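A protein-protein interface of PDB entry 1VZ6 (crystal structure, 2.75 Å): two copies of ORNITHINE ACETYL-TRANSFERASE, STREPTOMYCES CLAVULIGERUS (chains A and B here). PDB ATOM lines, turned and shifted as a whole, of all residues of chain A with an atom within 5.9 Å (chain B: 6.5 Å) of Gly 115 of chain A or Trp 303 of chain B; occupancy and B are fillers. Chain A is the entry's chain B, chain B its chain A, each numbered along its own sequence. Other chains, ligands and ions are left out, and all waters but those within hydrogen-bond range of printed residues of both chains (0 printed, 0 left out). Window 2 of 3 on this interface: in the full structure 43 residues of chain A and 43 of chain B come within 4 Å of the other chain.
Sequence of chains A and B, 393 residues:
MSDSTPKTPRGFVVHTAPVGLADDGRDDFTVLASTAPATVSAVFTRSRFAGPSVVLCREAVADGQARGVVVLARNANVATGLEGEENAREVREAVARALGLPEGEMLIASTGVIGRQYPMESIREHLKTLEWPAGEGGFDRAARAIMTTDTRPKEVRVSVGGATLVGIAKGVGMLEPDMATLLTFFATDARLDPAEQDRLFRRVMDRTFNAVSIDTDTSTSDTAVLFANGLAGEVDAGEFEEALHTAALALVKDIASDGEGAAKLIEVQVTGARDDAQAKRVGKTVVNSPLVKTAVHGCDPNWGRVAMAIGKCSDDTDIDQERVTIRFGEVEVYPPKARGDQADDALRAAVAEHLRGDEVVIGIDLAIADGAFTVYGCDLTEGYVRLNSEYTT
The backbone carbonyl oxygen (O) of Val 78 of chain A sits at hydrogen-bond distance from the backbone NH (N) of Gly 115 of chain A, 2.7 Å away. The backbone NH (N) of Ile 326 of chain B is in hydrogen-bond range of the backbone carbonyl oxygen (O) of Tyr 334 of chain B (2.9 Å). OD1 of Asn 302 of chain B sits close to N of Gly 304 of chain B (3.3 Å).
Ala 307 of chain B touches Phe 49 of chain A (O to CD1, 3.3 Å). OH of Tyr 334 of chain B touches CE2 of Phe 49 of chain A, 3.7 Å away. Ala 79 of chain A touches Trp 303 of chain B. Ile 114 of chain A touches Gly 304 of chain B. Gly 115 of chain A touches Trp 303 of chain B.
Printed residues of chain B within 4 Å of Ala 79 of chain A: Trp 303. Of the printed residues of chain B, Ile 114 of chain A touches Gly 304. Of chain B, only Trp 303 comes within 4 Å of Gly 115 of chain A. Printed residues of chain A within 4 Å of Trp 303 of chain B: Ala 79 (3.7 Å) and Gly 115 (3.7 Å). Of the printed residues of chain A, Gly 304 of chain B touches Ile 114 (3.8 Å). Of the printed residues of chain A, Tyr 334 of chain B touches Phe 49. The nearest residue of chain A that does not touch Trp 303 of chain B is Ile 114 of chain A (4.4 Å). The nearest printed residue of chain B that does not touch Ile 114 of chain A is Met 308 of chain B (4.2 Å).
Of the 15 printed residues of chain B, 4 touch a printed residue of chain A. Hydrophobic or aromatic side chains of chain B within 4 Å of the printed part of chain A: Trp 303, Ala 307 and Tyr 334. Printed residues of chain A that touch a printed residue of chain B: Phe 49, Ala 79, Ile 114 and Gly 115. Among the printed residues, 5 pairs touch across the chains.
No position is printed for both chains.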
ATOM      1  N   PHE A  49      31.145  16.560   8.939  1.00  0.00           N
ATOM      2  CA  PHE A  49      31.183  17.286   7.678  1.00  0.00           C
ATOM      3  C   PHE A  49      32.620  17.504   7.208  1.00  0.00           C
ATOM      4  O   PHE A  49      32.906  18.460   6.482  1.00  0.00           O
ATOM      5  CB  PHE A  49      30.477  18.640   7.811  1.00  0.00           C
ATOM      6  CG  PHE A  49      29.051  18.637   7.325  1.00  0.00           C
ATOM      7  CD1 PHE A  49      28.024  18.131   8.120  1.00  0.00           C
ATOM      8  CD2 PHE A  49      28.734  19.138   6.057  1.00  0.00           C
ATOM      9  CE1 PHE A  49      26.706  18.122   7.663  1.00  0.00           C
ATOM     10  CE2 PHE A  49      27.415  19.133   5.589  1.00  0.00           C
ATOM     11  CZ  PHE A  49      26.402  18.626   6.392  1.00  0.00           C
ATOM     12  N   ASN A  77      37.237  24.167   0.815  1.00  0.00           N
ATOM     13  CA  ASN A  77      36.856  23.125  -0.134  1.00  0.00           C
ATOM     14  C   ASN A  77      36.065  22.062   0.619  1.00  0.00           C
ATOM     15  O   ASN A  77      36.355  20.869   0.538  1.00  0.00           O
ATOM     16  CB  ASN A  77      38.076  22.483  -0.797  1.00  0.00           C
ATOM     17  CG  ASN A  77      37.682  21.448  -1.846  1.00  0.00           C
ATOM     18  OD1 ASN A  77      36.699  21.633  -2.570  1.00  0.00           O
ATOM     19  ND2 ASN A  77      38.446  20.364  -1.938  1.00  0.00           N
ATOM     20  N   VAL A  78      35.066  22.525   1.361  1.00  0.00           N
ATOM     21  CA  VAL A  78      34.203  21.666   2.151  1.00  0.00           C
ATOM     22  C   VAL A  78      32.767  21.769   1.625  1.00  0.00           C
ATOM     23  O   VAL A  78      32.336  22.836   1.172  1.00  0.00           O
ATOM     24  CB  VAL A  78      34.235  22.094   3.635  1.00  0.00           C
ATOM     25  CG1 VAL A  78      33.191  21.331   4.426  1.00  0.00           C
ATOM     26  CG2 VAL A  78      35.615  21.863   4.204  1.00  0.00           C
ATOM     27  N   ALA A  79      32.032  20.661   1.690  1.00  0.00           N
ATOM     28  CA  ALA A  79      30.649  20.629   1.227  1.00  0.00           C
ATOM     29  C   ALA A  79      30.587  21.092  -0.215  1.00  0.00           C
ATOM     30  O   ALA A  79      29.704  21.867  -0.591  1.00  0.00           O
ATOM     31  CB  ALA A  79      29.773  21.527   2.108  1.00  0.00           C
ATOM     32  N   THR A  80      31.533  20.615  -1.018  1.00  0.00           N
ATOM     33  CA  THR A  80      31.606  20.969  -2.430  1.00  0.00           C
ATOM     34  C   THR A  80      31.246  19.806  -3.368  1.00  0.00           C
ATOM     35  O   THR A  80      31.554  19.826  -4.566  1.00  0.00           O
ATOM     36  CB  THR A  80      33.007  21.485  -2.767  1.00  0.00           C
ATOM     37  OG1 THR A  80      33.985  20.657  -2.122  1.00  0.00           O
ATOM     38  CG2 THR A  80      33.167  22.924  -2.306  1.00  0.00           C
ATOM     39  N   VAL A 113      36.537  29.479   3.447  1.00  0.00           N
ATOM     40  CA  VAL A 113      35.088  29.396   3.240  1.00  0.00           C
ATOM     41  C   VAL A 113      34.570  27.996   2.920  1.00  0.00           C
ATOM     42  O   VAL A 113      35.247  27.202   2.274  1.00  0.00           O
ATOM     43  CB  VAL A 113      34.629  30.358   2.111  1.00  0.00           C
ATOM     44  CG1 VAL A 113      33.121  30.265   1.918  1.00  0.00           C
ATOM     45  CG2 VAL A 113      35.021  31.783   2.461  1.00  0.00           C
ATOM     46  N   ILE A 114      33.357  27.713   3.383  1.00  0.00           N
ATOM     47  CA  ILE A 114      32.711  26.426   3.159  1.00  0.00           C
ATOM     48  C   ILE A 114      31.682  26.517   2.018  1.00  0.00           C
ATOM     49  O   ILE A 114      31.025  27.545   1.831  1.00  0.00           O
ATOM     50  CB  ILE A 114      32.008  25.951   4.448  1.00  0.00           C
ATOM     51  CG1 ILE A 114      33.056  25.560   5.493  1.00  0.00           C
ATOM     52  CG2 ILE A 114      31.057  24.806   4.141  1.00  0.00           C
ATOM     53  CD1 ILE A 114      32.471  25.334   6.879  1.00  0.00           C
ATOM     54  N   GLY A 115      31.567  25.442   1.242  1.00  0.00           N
ATOM     55  CA  GLY A 115      30.615  25.417   0.145  1.00  0.00           C
ATOM     56  C   GLY A 115      30.937  26.285  -1.059  1.00  0.00           C
ATOM     57  O   GLY A 115      30.020  26.717  -1.759  1.00  0.00           O
ATOM     58  N   ARG A 116      32.220  26.544  -1.313  1.00  0.00           N
ATOM     59  CA  ARG A 116      32.616  27.362  -2.463  1.00  0.00           C
ATOM     60  C   ARG A 116      33.739  26.682  -3.252  1.00  0.00           C
ATOM     61  O   ARG A 116      34.873  26.616  -2.791  1.00  0.00           O
ATOM     62  CB  ARG A 116      33.059  28.758  -1.996  1.00  0.00           C
ATOM     63  N   GLN A 117      33.422  26.175  -4.440  1.00  0.00           N
ATOM     64  CA  GLN A 117      34.413  25.495  -5.270  1.00  0.00           C
ATOM     65  C   GLN A 117      35.694  26.311  -5.397  1.00  0.00           C
ATOM     66  O   GLN A 117      35.680  27.530  -5.245  1.00  0.00           O
ATOM     67  CB  GLN A 117      33.865  25.229  -6.676  1.00  0.00           C
ATOM     68  CG  GLN A 117      32.590  24.406  -6.755  1.00  0.00           C
ATOM     69  CD  GLN A 117      32.713  23.040  -6.103  1.00  0.00           C
ATOM     70  OE1 GLN A 117      33.765  22.398  -6.166  1.00  0.00           O
ATOM     71  NE2 GLN A 117      31.630  22.578  -5.485  1.00  0.00           N
ATOM     72  N   ASP B 300      22.596  36.725   7.535  1.00  0.00           N
ATOM     73  CA  ASP B 300      23.310  35.908   6.557  1.00  0.00           C
ATOM     74  C   ASP B 300      22.881  34.446   6.625  1.00  0.00           C
ATOM     75  O   ASP B 300      23.059  33.790   7.645  1.00  0.00           O
ATOM     76  CB  ASP B 300      24.822  36.042   6.808  1.00  0.00           C
ATOM     77  CG  ASP B 300      25.657  35.085   5.967  1.00  0.00           C
ATOM     78  OD1 ASP B 300      25.203  34.695   4.871  1.00  0.00           O
ATOM     79  OD2 ASP B 300      26.780  34.733   6.396  1.00  0.00           O
ATOM     80  N   PRO B 301      22.292  33.917   5.538  1.00  0.00           N
ATOM     81  CA  PRO B 301      21.835  32.522   5.484  1.00  0.00           C
ATOM     82  C   PRO B 301      22.993  31.564   5.235  1.00  0.00           C
ATOM     83  O   PRO B 301      22.999  30.812   4.268  1.00  0.00           O
ATOM     84  CB  PRO B 301      20.841  32.544   4.334  1.00  0.00           C
ATOM     85  CG  PRO B 301      21.483  33.512   3.392  1.00  0.00           C
ATOM     86  CD  PRO B 301      21.933  34.633   4.301  1.00  0.00           C
ATOM     87  N   ASN B 302      23.962  31.601   6.141  1.00  0.00           N
ATOM     88  CA  ASN B 302      25.177  30.791   6.078  1.00  0.00           C
ATOM     89  C   ASN B 302      24.945  29.307   6.404  1.00  0.00           C
ATOM     90  O   ASN B 302      25.207  28.878   7.530  1.00  0.00           O
ATOM     91  CB  ASN B 302      26.193  31.378   7.066  1.00  0.00           C
ATOM     92  CG  ASN B 302      27.620  31.090   6.683  1.00  0.00           C
ATOM     93  OD1 ASN B 302      27.990  29.950   6.394  1.00  0.00           O
ATOM     94  ND2 ASN B 302      28.444  32.129   6.691  1.00  0.00           N
ATOM     95  N   TRP B 303      24.473  28.514   5.440  1.00  0.00           N
ATOM     96  CA  TRP B 303      24.236  27.098   5.726  1.00  0.00           C
ATOM     97  C   TRP B 303      25.558  26.400   5.981  1.00  0.00           C
ATOM     98  O   TRP B 303      25.597  25.304   6.551  1.00  0.00           O
ATOM     99  CB  TRP B 303      23.484  26.394   4.583  1.00  0.00           C
ATOM    100  CG  TRP B 303      24.174  26.383   3.252  1.00  0.00           C
ATOM    101  CD1 TRP B 303      23.889  27.175   2.178  1.00  0.00           C
ATOM    102  CD2 TRP B 303      25.259  25.534   2.845  1.00  0.00           C
ATOM    103  NE1 TRP B 303      24.725  26.873   1.131  1.00  0.00           N
ATOM    104  CE2 TRP B 303      25.576  25.871   1.514  1.00  0.00           C
ATOM    105  CE3 TRP B 303      25.995  24.526   3.480  1.00  0.00           C
ATOM    106  CZ2 TRP B 303      26.597  25.233   0.800  1.00  0.00           C
ATOM    107  CZ3 TRP B 303      27.008  23.895   2.775  1.00  0.00           C
ATOM    108  CH2 TRP B 303      27.300  24.252   1.444  1.00  0.00           C
ATOM    109  N   GLY B 304      26.637  27.052   5.549  1.00  0.00           N
ATOM    110  CA  GLY B 304      27.964  26.504   5.739  1.00  0.00           C
ATOM    111  C   GLY B 304      28.270  26.370   7.213  1.00  0.00           C
ATOM    112  O   GLY B 304      28.775  25.342   7.660  1.00  0.00           O
ATOM    113  N   ARG B 305      27.965  27.408   7.983  1.00  0.00           N
ATOM    114  CA  ARG B 305      28.209  27.353   9.412  1.00  0.00           C
ATOM    115  C   ARG B 305      27.262  26.369  10.093  1.00  0.00           C
ATOM    116  O   ARG B 305      27.635  25.728  11.080  1.00  0.00           O
ATOM    117  CB  ARG B 305      28.089  28.747  10.012  1.00  0.00           C
ATOM    118  CG  ARG B 305      29.227  29.663   9.594  1.00  0.00           C
ATOM    119  CD  ARG B 305      29.071  31.035  10.200  1.00  0.00           C
ATOM    120  NE  ARG B 305      30.213  31.893   9.908  1.00  0.00           N
ATOM    121  CZ  ARG B 305      30.345  33.141  10.350  1.00  0.00           C
ATOM    122  NH1 ARG B 305      29.407  33.695  11.108  1.00  0.00           N
ATOM    123  NH2 ARG B 305      31.430  33.833  10.046  1.00  0.00           N
ATOM    124  N   VAL B 306      26.045  26.231   9.565  1.00  0.00           N
ATOM    125  CA  VAL B 306      25.090  25.278  10.133  1.00  0.00           C
ATOM    126  C   VAL B 306      25.647  23.869   9.920  1.00  0.00           C
ATOM    127  O   VAL B 306      25.604  23.029  10.816  1.00  0.00           O
ATOM    128  CB  VAL B 306      23.692  25.390   9.464  1.00  0.00           C
ATOM    129  CG1 VAL B 306      22.792  24.270   9.953  1.00  0.00           C
ATOM    130  CG2 VAL B 306      23.058  26.734   9.796  1.00  0.00           C
ATOM    131  N   ALA B 307      26.183  23.627   8.727  1.00  0.00           N
ATOM    132  CA  ALA B 307      26.779  22.341   8.390  1.00  0.00           C
ATOM    133  C   ALA B 307      27.928  22.032   9.365  1.00  0.00           C
ATOM    134  O   ALA B 307      28.009  20.933   9.922  1.00  0.00           O
ATOM    135  CB  ALA B 307      27.288  22.378   6.961  1.00  0.00           C
ATOM    136  N   MET B 308      28.811  23.012   9.558  1.00  0.00           N
ATOM    137  CA  MET B 308      29.938  22.891  10.479  1.00  0.00           C
ATOM    138  C   MET B 308      29.394  22.514  11.855  1.00  0.00           C
ATOM    139  O   MET B 308      29.920  21.619  12.519  1.00  0.00           O
ATOM    140  CB  MET B 308      30.683  24.229  10.550  1.00  0.00           C
ATOM    141  CG  MET B 308      31.758  24.353  11.638  1.00  0.00           C
ATOM    142  SD  MET B 308      31.133  24.649  13.326  1.00  0.00           S
ATOM    143  CE  MET B 308      30.341  26.259  13.144  1.00  0.00           C
ATOM    144  N   ILE B 326      19.389  21.000   4.678  1.00  0.00           N
ATOM    145  CA  ILE B 326      19.240  22.184   5.518  1.00  0.00           C
ATOM    146  C   ILE B 326      18.357  23.210   4.815  1.00  0.00           C
ATOM    147  O   ILE B 326      18.455  23.406   3.601  1.00  0.00           O
ATOM    148  CB  ILE B 326      20.617  22.852   5.811  1.00  0.00           C
ATOM    149  CG1 ILE B 326      21.562  21.840   6.461  1.00  0.00           C
ATOM    150  CG2 ILE B 326      20.434  24.071   6.712  1.00  0.00           C
ATOM    151  CD1 ILE B 326      22.998  22.302   6.495  1.00  0.00           C
ATOM    152  N   PHE B 328      16.266  27.248   5.335  1.00  0.00           N
ATOM    153  CA  PHE B 328      16.048  28.479   6.076  1.00  0.00           C
ATOM    154  C   PHE B 328      14.619  28.860   5.735  1.00  0.00           C
ATOM    155  O   PHE B 328      14.300  29.162   4.587  1.00  0.00           O
ATOM    156  CB  PHE B 328      17.021  29.571   5.623  1.00  0.00           C
ATOM    157  CG  PHE B 328      18.401  29.417   6.184  1.00  0.00           C
ATOM    158  CD1 PHE B 328      18.607  29.422   7.556  1.00  0.00           C
ATOM    159  CD2 PHE B 328      19.498  29.272   5.341  1.00  0.00           C
ATOM    160  CE1 PHE B 328      19.887  29.284   8.086  1.00  0.00           C
ATOM    161  CE2 PHE B 328      20.787  29.132   5.865  1.00  0.00           C
ATOM    162  CZ  PHE B 328      20.979  29.139   7.241  1.00  0.00           C
ATOM    163  N   VAL B 333      18.366  24.947   1.289  1.00  0.00           N
ATOM    164  CA  VAL B 333      19.574  25.551   0.755  1.00  0.00           C
ATOM    165  C   VAL B 333      20.729  24.554   0.640  1.00  0.00           C
ATOM    166  O   VAL B 333      21.741  24.832  -0.012  1.00  0.00           O
ATOM    167  CB  VAL B 333      19.993  26.760   1.624  1.00  0.00           C
ATOM    168  CG1 VAL B 333      18.882  27.797   1.617  1.00  0.00           C
ATOM    169  CG2 VAL B 333      20.283  26.313   3.051  1.00  0.00           C
ATOM    170  N   TYR B 334      20.568  23.392   1.273  1.00  0.00           N
ATOM    171  CA  TYR B 334      21.579  22.340   1.228  1.00  0.00           C
ATOM    172  C   TYR B 334      20.923  20.960   1.108  1.00  0.00           C
ATOM    173  O   TYR B 334      20.039  20.617   1.888  1.00  0.00           O
ATOM    174  CB  TYR B 334      22.455  22.365   2.481  1.00  0.00           C
ATOM    175  CG  TYR B 334      23.491  21.263   2.476  1.00  0.00           C
ATOM    176  CD1 TYR B 334      24.666  21.391   1.740  1.00  0.00           C
ATOM    177  CD2 TYR B 334      23.267  20.061   3.151  1.00  0.00           C
ATOM    178  CE1 TYR B 334      25.592  20.349   1.671  1.00  0.00           C
ATOM    179  CE2 TYR B 334      24.191  19.012   3.087  1.00  0.00           C
ATOM    180  CZ  TYR B 334      25.346  19.163   2.345  1.00  0.00           C
ATOM    181  OH  TYR B 334      26.252  18.130   2.265  1.00  0.00           O
ATOM    182  N   PRO B 335      21.351  20.150   0.124  1.00  0.00           N
ATOM    183  CA  PRO B 335      22.396  20.422  -0.872  1.00  0.00           C
ATOM    184  C   PRO B 335      22.042  21.584  -1.798  1.00  0.00           C
ATOM    185  O   PRO B 335      20.874  21.803  -2.110  1.00  0.00           O
ATOM    186  CB  PRO B 335      22.492  19.107  -1.641  1.00  0.00           C
ATOM    187  CG  PRO B 335      22.052  18.090  -0.639  1.00  0.00           C
ATOM    188  CD  PRO B 335      20.872  18.765  -0.002  1.00  0.00           C
ATOM    189  N   PRO B 336      23.057  22.334  -2.256  1.00  0.00           N
ATOM    190  CA  PRO B 336      22.902  23.486  -3.151  1.00  0.00           C
ATOM    191  C   PRO B 336      22.092  23.147  -4.395  1.00  0.00           C
ATOM    192  O   PRO B 336      22.362  22.145  -5.055  1.00  0.00           O
ATOM    193  CB  PRO B 336      24.338  23.843  -3.496  1.00  0.00           C
ATOM    194  CG  PRO B 336      25.085  23.444  -2.261  1.00  0.00           C
ATOM    195  CD  PRO B 336      24.477  22.109  -1.939  1.00  0.00           C
